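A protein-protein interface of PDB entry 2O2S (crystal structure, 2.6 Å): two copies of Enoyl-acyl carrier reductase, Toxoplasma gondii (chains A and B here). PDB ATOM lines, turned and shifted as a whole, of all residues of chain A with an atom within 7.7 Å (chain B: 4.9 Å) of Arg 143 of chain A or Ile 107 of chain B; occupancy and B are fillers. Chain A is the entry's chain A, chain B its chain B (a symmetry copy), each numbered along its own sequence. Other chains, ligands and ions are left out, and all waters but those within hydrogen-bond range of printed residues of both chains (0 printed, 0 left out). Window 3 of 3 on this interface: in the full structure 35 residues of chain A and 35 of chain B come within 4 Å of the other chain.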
ATOM      1  N   GLU A 133      34.792  23.948 -24.168  1.00  0.00           N
ATOM      2  CA  GLU A 133      34.959  22.486 -24.022  1.00  0.00           C
ATOM      3  C   GLU A 133      36.060  21.939 -24.894  1.00  0.00           C
ATOM      4  O   GLU A 133      36.073  20.778 -25.253  1.00  0.00           O
ATOM      5  CB  GLU A 133      33.635  21.740 -24.266  1.00  0.00           C
ATOM      6  CG  GLU A 133      32.566  22.093 -23.253  1.00  0.00           C
ATOM      7  CD  GLU A 133      31.196  21.481 -23.536  1.00  0.00           C
ATOM      8  OE1 GLU A 133      31.096  20.462 -24.256  1.00  0.00           O
ATOM      9  OE2 GLU A 133      30.207  22.026 -22.997  1.00  0.00           O
ATOM     10  N   GLU A 140      32.065  14.023 -26.923  1.00  0.00           N
ATOM     11  CA  GLU A 140      31.807  14.413 -25.545  1.00  0.00           C
ATOM     12  C   GLU A 140      31.622  15.914 -25.412  1.00  0.00           C
ATOM     13  O   GLU A 140      31.808  16.484 -24.349  1.00  0.00           O
ATOM     14  CB  GLU A 140      32.972  13.960 -24.667  1.00  0.00           C
ATOM     15  CG  GLU A 140      33.000  12.482 -24.510  1.00  0.00           C
ATOM     16  CD  GLU A 140      34.304  11.965 -24.008  1.00  0.00           C
ATOM     17  OE1 GLU A 140      35.134  12.768 -23.556  1.00  0.00           O
ATOM     18  OE2 GLU A 140      34.484  10.741 -24.041  1.00  0.00           O
ATOM     19  N   THR A 141      31.240  16.551 -26.503  1.00  0.00           N
ATOM     20  CA  THR A 141      31.052  17.977 -26.550  1.00  0.00           C
ATOM     21  C   THR A 141      29.558  18.286 -26.652  1.00  0.00           C
ATOM     22  O   THR A 141      28.768  17.547 -27.267  1.00  0.00           O
ATOM     23  CB  THR A 141      31.829  18.534 -27.726  1.00  0.00           C
ATOM     24  OG1 THR A 141      33.210  18.156 -27.588  1.00  0.00           O
ATOM     25  CG2 THR A 141      31.676  20.054 -27.825  1.00  0.00           C
ATOM     26  N   SER A 142      29.177  19.380 -26.014  1.00  0.00           N
ATOM     27  CA  SER A 142      27.797  19.777 -25.888  1.00  0.00           C
ATOM     28  C   SER A 142      27.434  20.819 -26.944  1.00  0.00           C
ATOM     29  O   SER A 142      28.294  21.500 -27.484  1.00  0.00           O
ATOM     30  CB  SER A 142      27.573  20.353 -24.497  1.00  0.00           C
ATOM     31  OG  SER A 142      28.205  21.602 -24.378  1.00  0.00           O
ATOM     32  N   ARG A 143      26.144  20.923 -27.214  1.00  0.00           N
ATOM     33  CA  ARG A 143      25.607  21.925 -28.092  1.00  0.00           C
ATOM     34  C   ARG A 143      25.951  23.335 -27.562  1.00  0.00           C
ATOM     35  O   ARG A 143      26.306  24.228 -28.318  1.00  0.00           O
ATOM     36  CB  ARG A 143      24.100  21.714 -28.192  1.00  0.00           C
ATOM     37  CG  ARG A 143      23.443  22.519 -29.256  1.00  0.00           C
ATOM     38  CD  ARG A 143      21.951  22.188 -29.421  1.00  0.00           C
ATOM     39  NE  ARG A 143      21.690  20.795 -29.843  1.00  0.00           N
ATOM     40  CZ  ARG A 143      21.370  20.377 -31.075  1.00  0.00           C
ATOM     41  NH1 ARG A 143      21.229  21.237 -32.087  1.00  0.00           N
ATOM     42  NH2 ARG A 143      21.186  19.065 -31.289  1.00  0.00           N
ATOM     43  N   LYS A 144      25.866  23.533 -26.247  1.00  0.00           N
ATOM     44  CA  LYS A 144      26.071  24.877 -25.668  1.00  0.00           C
ATOM     45  C   LYS A 144      27.516  25.330 -25.888  1.00  0.00           C
ATOM     46  O   LYS A 144      27.751  26.513 -26.209  1.00  0.00           O
ATOM     47  CB  LYS A 144      25.686  24.897 -24.182  1.00  0.00           C
ATOM     48  CG  LYS A 144      26.082  26.154 -23.369  1.00  0.00           C
ATOM     49  CD  LYS A 144      25.409  26.157 -21.966  1.00  0.00           C
ATOM     50  CE  LYS A 144      25.567  27.496 -21.194  1.00  0.00           C
ATOM     51  NZ  LYS A 144      26.764  27.485 -20.315  1.00  0.00           N
ATOM     52  N   GLY A 145      28.454  24.378 -25.763  1.00  0.00           N
ATOM     53  CA  GLY A 145      29.879  24.643 -25.854  1.00  0.00           C
ATOM     54  C   GLY A 145      30.434  24.668 -27.261  1.00  0.00           C
ATOM     55  O   GLY A 145      31.383  25.402 -27.566  1.00  0.00           O
ATOM     56  N   TYR A 146      29.873  23.822 -28.116  1.00  0.00           N
ATOM     57  CA  TYR A 146      30.255  23.787 -29.526  1.00  0.00           C
ATOM     58  C   TYR A 146      29.763  25.094 -30.162  1.00  0.00           C
ATOM     59  O   TYR A 146      30.479  25.744 -30.925  1.00  0.00           O
ATOM     60  CB  TYR A 146      29.632  22.541 -30.157  1.00  0.00           C
ATOM     61  CG  TYR A 146      29.719  22.364 -31.673  1.00  0.00           C
ATOM     62  CD1 TYR A 146      30.477  21.333 -32.218  1.00  0.00           C
ATOM     63  CD2 TYR A 146      28.988  23.172 -32.548  1.00  0.00           C
ATOM     64  CE1 TYR A 146      30.547  21.122 -33.583  1.00  0.00           C
ATOM     65  CE2 TYR A 146      29.054  22.970 -33.931  1.00  0.00           C
ATOM     66  CZ  TYR A 146      29.843  21.939 -34.448  1.00  0.00           C
ATOM     67  OH  TYR A 146      29.924  21.715 -35.812  1.00  0.00           O
ATOM     68  N   LEU A 147      28.548  25.487 -29.800  1.00  0.00           N
ATOM     69  CA  LEU A 147      27.956  26.705 -30.332  1.00  0.00           C
ATOM     70  C   LEU A 147      28.712  27.920 -29.876  1.00  0.00           C
ATOM     71  O   LEU A 147      28.919  28.817 -30.647  1.00  0.00           O
ATOM     72  CB  LEU A 147      26.461  26.791 -29.990  1.00  0.00           C
ATOM     73  CG  LEU A 147      25.641  25.802 -30.856  1.00  0.00           C
ATOM     74  CD1 LEU A 147      24.165  25.826 -30.488  1.00  0.00           C
ATOM     75  CD2 LEU A 147      25.831  26.023 -32.376  1.00  0.00           C
ATOM     76  N   ALA A 148      29.130  27.924 -28.625  1.00  0.00           N
ATOM     77  CA  ALA A 148      30.034  28.913 -28.082  1.00  0.00           C
ATOM     78  C   ALA A 148      31.345  28.979 -28.863  1.00  0.00           C
ATOM     79  O   ALA A 148      31.861  30.068 -29.150  1.00  0.00           O
ATOM     80  CB  ALA A 148      30.330  28.574 -26.607  1.00  0.00           C
ATOM     81  N   ALA A 149      31.919  27.829 -29.193  1.00  0.00           N
ATOM     82  CA  ALA A 149      33.172  27.828 -29.921  1.00  0.00           C
ATOM     83  C   ALA A 149      32.992  28.565 -31.245  1.00  0.00           C
ATOM     84  O   ALA A 149      33.824  29.419 -31.582  1.00  0.00           O
ATOM     85  CB  ALA A 149      33.692  26.411 -30.137  1.00  0.00           C
ATOM     86  N   LEU B  79      11.123  13.725 -34.142  1.00  0.00           N
ATOM     87  CA  LEU B  79      12.539  14.020 -34.005  1.00  0.00           C
ATOM     88  C   LEU B  79      12.802  15.447 -34.404  1.00  0.00           C
ATOM     89  O   LEU B  79      12.613  15.837 -35.545  1.00  0.00           O
ATOM     90  CB  LEU B  79      13.377  13.057 -34.842  1.00  0.00           C
ATOM     91  CG  LEU B  79      14.917  13.051 -34.799  1.00  0.00           C
ATOM     92  CD1 LEU B  79      15.476  13.948 -35.882  1.00  0.00           C
ATOM     93  CD2 LEU B  79      15.534  13.407 -33.438  1.00  0.00           C
ATOM     94  N   ASP B  80      13.194  16.228 -33.411  1.00  0.00           N
ATOM     95  CA  ASP B  80      13.670  17.562 -33.612  1.00  0.00           C
ATOM     96  C   ASP B  80      15.140  17.589 -33.189  1.00  0.00           C
ATOM     97  O   ASP B  80      15.464  17.666 -32.007  1.00  0.00           O
ATOM     98  CB  ASP B  80      12.836  18.549 -32.801  1.00  0.00           C
ATOM     99  CG  ASP B  80      13.132  19.961 -33.169  1.00  0.00           C
ATOM    100  OD1 ASP B  80      12.176  20.729 -33.328  1.00  0.00           O
ATOM    101  OD2 ASP B  80      14.326  20.290 -33.338  1.00  0.00           O
ATOM    102  N   ALA B  81      16.027  17.515 -34.177  1.00  0.00           N
ATOM    103  CA  ALA B  81      17.471  17.442 -33.938  1.00  0.00           C
ATOM    104  C   ALA B  81      18.079  18.793 -33.556  1.00  0.00           C
ATOM    105  O   ALA B  81      19.281  18.935 -33.548  1.00  0.00           O
ATOM    106  CB  ALA B  81      18.184  16.865 -35.169  1.00  0.00           C
ATOM    107  N   ALA B  82      17.250  19.790 -33.264  1.00  0.00           N
ATOM    108  CA  ALA B  82      17.714  20.989 -32.561  1.00  0.00           C
ATOM    109  C   ALA B  82      17.720  20.816 -31.010  1.00  0.00           C
ATOM    110  O   ALA B  82      18.164  21.720 -30.261  1.00  0.00           O
ATOM    111  CB  ALA B  82      16.865  22.207 -32.971  1.00  0.00           C
ATOM    112  N   PHE B  83      17.223  19.672 -30.532  1.00  0.00           N
ATOM    113  CA  PHE B  83      17.199  19.398 -29.106  1.00  0.00           C
ATOM    114  C   PHE B  83      17.823  18.043 -28.805  1.00  0.00           C
ATOM    115  O   PHE B  83      17.435  17.007 -29.342  1.00  0.00           O
ATOM    116  CB  PHE B  83      15.773  19.479 -28.576  1.00  0.00           C
ATOM    117  CG  PHE B  83      15.062  20.741 -28.966  1.00  0.00           C
ATOM    118  CD1 PHE B  83      13.940  20.708 -29.781  1.00  0.00           C
ATOM    119  CD2 PHE B  83      15.512  21.967 -28.517  1.00  0.00           C
ATOM    120  CE1 PHE B  83      13.273  21.896 -30.139  1.00  0.00           C
ATOM    121  CE2 PHE B  83      14.839  23.156 -28.865  1.00  0.00           C
ATOM    122  CZ  PHE B  83      13.733  23.115 -29.690  1.00  0.00           C
ATOM    123  N   ASP B  84      18.805  18.083 -27.914  1.00  0.00           N
ATOM    124  CA  ASP B  84      19.527  16.882 -27.466  1.00  0.00           C
ATOM    125  C   ASP B  84      18.745  16.105 -26.428  1.00  0.00           C
ATOM    126  O   ASP B  84      18.728  14.862 -26.444  1.00  0.00           O
ATOM    127  CB  ASP B  84      20.858  17.287 -26.867  1.00  0.00           C
ATOM    128  CG  ASP B  84      21.717  18.051 -27.841  1.00  0.00           C
ATOM    129  OD1 ASP B  84      21.884  17.542 -28.965  1.00  0.00           O
ATOM    130  OD2 ASP B  84      22.209  19.147 -27.494  1.00  0.00           O
ATOM    131  N   TYR B 105      10.892  13.370 -28.594  1.00  0.00           N
ATOM    132  CA  TYR B 105      11.392  13.792 -29.901  1.00  0.00           C
ATOM    133  C   TYR B 105      12.812  14.423 -29.868  1.00  0.00           C
ATOM    134  O   TYR B 105      13.343  14.798 -30.909  1.00  0.00           O
ATOM    135  CB  TYR B 105      10.356  14.705 -30.602  1.00  0.00           C
ATOM    136  CG  TYR B 105       9.902  15.912 -29.802  1.00  0.00           C
ATOM    137  CD1 TYR B 105      10.720  17.019 -29.676  1.00  0.00           C
ATOM    138  CD2 TYR B 105       8.657  15.946 -29.169  1.00  0.00           C
ATOM    139  CE1 TYR B 105      10.313  18.151 -28.934  1.00  0.00           C
ATOM    140  CE2 TYR B 105       8.240  17.077 -28.415  1.00  0.00           C
ATOM    141  CZ  TYR B 105       9.082  18.173 -28.310  1.00  0.00           C
ATOM    142  OH  TYR B 105       8.747  19.298 -27.597  1.00  0.00           O
ATOM    143  N   THR B 106      13.447  14.508 -28.701  1.00  0.00           N
ATOM    144  CA  THR B 106      14.868  14.879 -28.652  1.00  0.00           C
ATOM    145  C   THR B 106      15.756  13.704 -29.070  1.00  0.00           C
ATOM    146  O   THR B 106      15.360  12.550 -28.997  1.00  0.00           O
ATOM    147  CB  THR B 106      15.310  15.376 -27.260  1.00  0.00           C
ATOM    148  OG1 THR B 106      15.260  14.307 -26.309  1.00  0.00           O
ATOM    149  CG2 THR B 106      14.416  16.529 -26.795  1.00  0.00           C
ATOM    150  N   ILE B 107      16.975  14.023 -29.486  1.00  0.00           N
ATOM    151  CA  ILE B 107      17.904  13.047 -30.022  1.00  0.00           C
ATOM    152  C   ILE B 107      18.179  11.958 -28.984  1.00  0.00           C
ATOM    153  O   ILE B 107      18.223  10.764 -29.334  1.00  0.00           O
ATOM    154  CB  ILE B 107      19.231  13.737 -30.510  1.00  0.00           C
ATOM    155  CG1 ILE B 107      18.943  14.697 -31.681  1.00  0.00           C
ATOM    156  CG2 ILE B 107      20.300  12.699 -30.912  1.00  0.00           C
ATOM    157  CD1 ILE B 107      19.966  15.799 -31.836  1.00  0.00           C
ATOM    158  N   LYS B 108      18.342  12.347 -27.714  1.00  0.00           N
ATOM    159  CA  LYS B 108      18.589  11.345 -26.675  1.00  0.00           C
ATOM    160  C   LYS B 108      17.422  10.381 -26.556  1.00  0.00           C
ATOM    161  O   LYS B 108      17.629   9.169 -26.355  1.00  0.00           O
ATOM    162  CB  LYS B 108      18.856  11.954 -25.293  1.00  0.00           C
ATOM    163  CG  LYS B 108      19.214  10.866 -24.242  1.00  0.00           C
ATOM    164  CD  LYS B 108      19.955  11.413 -23.014  1.00  0.00           C
ATOM    165  CE  LYS B 108      20.632  10.265 -22.209  1.00  0.00           C
ATOM    166  NZ  LYS B 108      21.552  10.744 -21.103  1.00  0.00           N
ATOM    167  N   GLU B 109      16.209  10.929 -26.671  1.00  0.00           N
ATOM    168  CA  GLU B 109      14.990  10.162 -26.453  1.00  0.00           C
ATOM    169  C   GLU B 109      14.673   9.281 -27.644  1.00  0.00           C
ATOM    170  O   GLU B 109      14.163   8.170 -27.479  1.00  0.00           O
ATOM    171  CB  GLU B 109      13.806  11.097 -26.175  1.00  0.00           C
ATOM    172  CG  GLU B 109      13.837  11.805 -24.834  1.00  0.00           C
ATOM    173  CD  GLU B 109      12.685  12.793 -24.666  1.00  0.00           C
ATOM    174  OE1 GLU B 109      12.333  13.534 -25.629  1.00  0.00           O
ATOM    175  OE2 GLU B 109      12.125  12.830 -23.553  1.00  0.00           O
ATOM    176  N   VAL B 110      14.961   9.768 -28.847  1.00  0.00           N
ATOM    177  CA  VAL B 110      14.707   8.967 -30.044  1.00  0.00           C
ATOM    178  C   VAL B 110      15.682   7.795 -30.102  1.00  0.00           C
ATOM    179  O   VAL B 110      15.320   6.702 -30.521  1.00  0.00           O
ATOM    180  CB  VAL B 110      14.787   9.795 -31.330  1.00  0.00           C
ATOM    181  CG1 VAL B 110      14.652   8.899 -32.538  1.00  0.00           C
ATOM    182  CG2 VAL B 110      13.707  10.846 -31.335  1.00  0.00           C
ATOM    183  N   ALA B 111      16.917   8.034 -29.678  1.00  0.00           N
ATOM    184  CA  ALA B 111      17.923   6.976 -29.616  1.00  0.00           C
ATOM    185  C   ALA B 111      17.453   5.864 -28.700  1.00  0.00           C
ATOM    186  O   ALA B 111      17.500   4.669 -29.047  1.00  0.00           O
ATOM    187  CB  ALA B 111      19.243   7.535 -29.113  1.00  0.00           C
ATOM    188  N   SER B 151      23.712  25.020 -35.401  1.00  0.00           N
ATOM    189  CA  SER B 151      23.006  24.147 -34.503  1.00  0.00           C
ATOM    190  C   SER B 151      22.122  23.138 -35.231  1.00  0.00           C
ATOM    191  O   SER B 151      22.186  21.949 -34.934  1.00  0.00           O
ATOM    192  CB  SER B 151      22.196  24.970 -33.534  1.00  0.00           C
ATOM    193  OG  SER B 151      21.839  24.145 -32.465  1.00  0.00           O
ATOM    194  N   ASN B 152      21.307  23.593 -36.185  1.00  0.00           N
ATOM    195  CA  ASN B 152      20.385  22.663 -36.916  1.00  0.00           C
ATOM    196  C   ASN B 152      21.092  21.713 -37.852  1.00  0.00           C
ATOM    197  O   ASN B 152      20.740  20.568 -37.951  1.00  0.00           O
ATOM    198  CB  ASN B 152      19.350  23.421 -37.747  1.00  0.00           C
ATOM    199  CG  ASN B 152      18.375  24.226 -36.891  1.00  0.00           C
ATOM    200  OD1 ASN B 152      17.861  23.739 -35.888  1.00  0.00           O
ATOM    201  ND2 ASN B 152      18.108  25.453 -37.304  1.00  0.00           N
ATOM    202  N   TYR B 155      25.745  20.622 -35.655  1.00  0.00           N
ATOM    203  CA  TYR B 155      25.819  19.983 -34.342  1.00  0.00           C
ATOM    204  C   TYR B 155      24.884  18.787 -34.313  1.00  0.00           C
ATOM    205  O   TYR B 155      25.277  17.707 -33.876  1.00  0.00           O
ATOM    206  CB  TYR B 155      25.539  20.902 -33.155  1.00  0.00           C
ATOM    207  CG  TYR B 155      25.812  20.170 -31.844  1.00  0.00           C
ATOM    208  CD1 TYR B 155      27.086  20.047 -31.356  1.00  0.00           C
ATOM    209  CD2 TYR B 155      24.798  19.557 -31.132  1.00  0.00           C
ATOM    210  CE1 TYR B 155      27.336  19.359 -30.177  1.00  0.00           C
ATOM    211  CE2 TYR B 155      25.038  18.866 -29.950  1.00  0.00           C
ATOM    212  CZ  TYR B 155      26.300  18.770 -29.485  1.00  0.00           C
ATOM    213  OH  TYR B 155      26.566  18.111 -28.334  1.00  0.00           O
ATOM    214  N   SER B 156      23.670  18.969 -34.805  1.00  0.00           N
ATOM    215  CA  SER B 156      22.741  17.836 -35.069  1.00  0.00           C
ATOM    216  C   SER B 156      23.397  16.490 -35.469  1.00  0.00           C
ATOM    217  O   SER B 156      22.952  15.418 -35.038  1.00  0.00           O
ATOM    218  CB  SER B 156      21.724  18.232 -36.154  1.00  0.00           C
ATOM    219  OG  SER B 156      22.373  18.543 -37.372  1.00  0.00           O
ATOM    220  N   SER B 159      25.532  15.225 -32.477  1.00  0.00           N
ATOM    221  CA  SER B 159      24.638  14.759 -31.430  1.00  0.00           C
ATOM    222  C   SER B 159      24.108  13.404 -31.791  1.00  0.00           C
ATOM    223  O   SER B 159      24.030  12.532 -30.955  1.00  0.00           O
ATOM    224  CB  SER B 159      23.492  15.718 -31.260  1.00  0.00           C
ATOM    225  OG  SER B 159      22.722  15.360 -30.140  1.00  0.00           O
ATOM    226  N   LEU B 160      23.771  13.213 -33.058  1.00  0.00           N
ATOM    227  CA  LEU B 160      23.281  11.936 -33.507  1.00  0.00           C
ATOM    228  C   LEU B 160      24.296  10.839 -33.321  1.00  0.00           C
ATOM    229  O   LEU B 160      23.967   9.723 -32.956  1.00  0.00           O
ATOM    230  CB  LEU B 160      22.975  12.017 -34.977  1.00  0.00           C
ATOM    231  CG  LEU B 160      21.561  12.408 -35.337  1.00  0.00           C
ATOM    232  CD1 LEU B 160      21.522  12.643 -36.797  1.00  0.00           C
ATOM    233  CD2 LEU B 160      20.591  11.301 -34.943  1.00  0.00           C
ATOM    234  N   HIS B 163      24.676   9.934 -29.720  1.00  0.00           N
ATOM    235  CA  HIS B 163      23.605   9.148 -29.077  1.00  0.00           C
ATOM    236  C   HIS B 163      23.277   7.838 -29.797  1.00  0.00           C
ATOM    237  O   HIS B 163      22.645   6.959 -29.222  1.00  0.00           O
ATOM    238  CB  HIS B 163      22.343   9.982 -28.902  1.00  0.00           C
ATOM    239  CG  HIS B 163      22.499  11.105 -27.936  1.00  0.00           C
ATOM    240  ND1 HIS B 163      22.311  10.948 -26.577  1.00  0.00           N
ATOM    241  CD2 HIS B 163      22.824  12.402 -28.122  1.00  0.00           C
ATOM    242  CE1 HIS B 163      22.528  12.097 -25.967  1.00  0.00           C
ATOM    243  NE2 HIS B 163      22.822  13.000 -26.884  1.00  0.00           N
ATOM    244  N   PHE B 164      23.705   7.699 -31.041  1.00  0.00           N
ATOM    245  CA  PHE B 164      23.431   6.484 -31.760  1.00  0.00           C
ATOM    246  C   PHE B 164      24.627   5.573 -31.810  1.00  0.00           C
ATOM    247  O   PHE B 164      24.466   4.362 -31.902  1.00  0.00           O
ATOM    248  CB  PHE B 164      22.924   6.781 -33.162  1.00  0.00           C
ATOM    249  CG  PHE B 164      21.435   6.966 -33.221  1.00  0.00           C
ATOM    250  CD1 PHE B 164      20.870   8.228 -33.105  1.00  0.00           C
ATOM    251  CD2 PHE B 164      20.605   5.875 -33.368  1.00  0.00           C
ATOM    252  CE1 PHE B 164      19.512   8.392 -33.152  1.00  0.00           C
ATOM    253  CE2 PHE B 164      19.232   6.038 -33.408  1.00  0.00           C
ATOM    254  CZ  PHE B 164      18.689   7.299 -33.295  1.00  0.00           C
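Among the printed residues, pairs that only touch across the chains: Ser 142 of chain A with Tyr 155 of chain B (3.2 Å), Arg 143 of chain A with Ala 82 of chain B (3.6 Å), Arg 143 of chain A with Ile 107 of chain B (3.5 Å), Tyr 146 of chain A with Tyr 155 of chain B (3.5 Å) and Leu 147 of chain A with Ser 151 of chain B (3.5 Å).
The side-chain hydroxyl of Tyr 155 of chain B lies within hydrogen-bond range of the backbone carbonyl oxygen of Thr 141 of chain A. The guanidinium group (NH2) of Arg 143 of chain A lies within hydrogen-bond range of the backbone carbonyl oxygen (O) of Ala 81 of chain B (3.0 Å). NH2 of Arg 143 of chain A is in salt-bridge range of OD1 of Asp 84 of chain B. NH1 of Arg 143 of chain A is in hydrogen-bond range of OG of Ser 151 of chain B. The side-chain hydroxyl of Tyr 155 of chain B sits at hydrogen-bond distance from the backbone NH of Arg 143 of chain A.
The side-chain carboxylate (OE2) of Glu 133 of chain A sits at hydrogen-bond distance from the side-chain hydroxyl (OG) of Ser 142 of chain A (2.5 Å). The side-chain hydroxyl (OG) of Ser 142 of chain A is in hydrogen-bond range of the backbone NH (N) of Gly 145 of chain A, 3.1 Å away. The side-chain carboxylate of Asp 80 of chain B sits at hydrogen-bond distance from the backbone NH of Ala 82 of chain B (3.0 Å). O of Phe 83 of chain B is in hydrogen-bond range of N of Ile 107 of chain B (3.0 Å). OD1 of Asp 84 of chain B sits at hydrogen-bond distance from OG of Ser 159 of chain B. O of Ser 151 of chain B lies within hydrogen-bond range of N of Ser 156 of chain B.
Of the 11 printed residues of chain A, 5 touch a printed residue of chain B. Printed residues of chain A that touch a printed residue of chain B: Thr 141, Ser 142, Arg 143, Tyr 146 and Leu 147. Hydrophobic or aromatic side chains of chain A that line the printed part of chain B: Tyr 146 and Leu 147. Of the 21 printed residues of chain B, 6 touch a printed residue of chain A. Printed residues of chain B that touch a printed residue of chain A: Ala 81, Ala 82, Asp 84, Ile 107, Ser 151 and Tyr 155. Among the printed residues, Asp or Glu carboxylates within 4 Å of a Lys or Arg side-chain nitrogen of the other chain: Arg 143 of chain A with Asp 84 of chain B.
Of chain B, only Ala 81 (3.0 Å), Ala 82 (3.6 Å), Asp 84 (2.9 Å), Ile 107 (3.5 Å), Ser 151 (3.0 Å) and Tyr 155 (3.1 Å) come within 4 Å of Arg 143 of chain A. Printed residues of chain B within 4 Å of Tyr 146 of chain A: Tyr 155. Of the printed residues of chain A, Ala 81 of chain B touches Arg 143 (3.0 Å). Printed residues of chain A within 4 Å of Asp 84 of chain B: Arg 143. Ile 107 of chain B touches one residue of chain A. Ala 111 of chain B touches none of the printed residues of chain A. The nearest printed residue of chain A that does not touch Ile 107 of chain B is Thr 141 of chain A (10.1 Å). The nearest printed residue of chain A that does not touch Asp 84 of chain B is Ser 142 of chain A (5.5 Å).
No position is printed for both chains. Of the 10 pairs that touch across the chains among the printed residues, none has its exchanged pair printed and touching as well.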
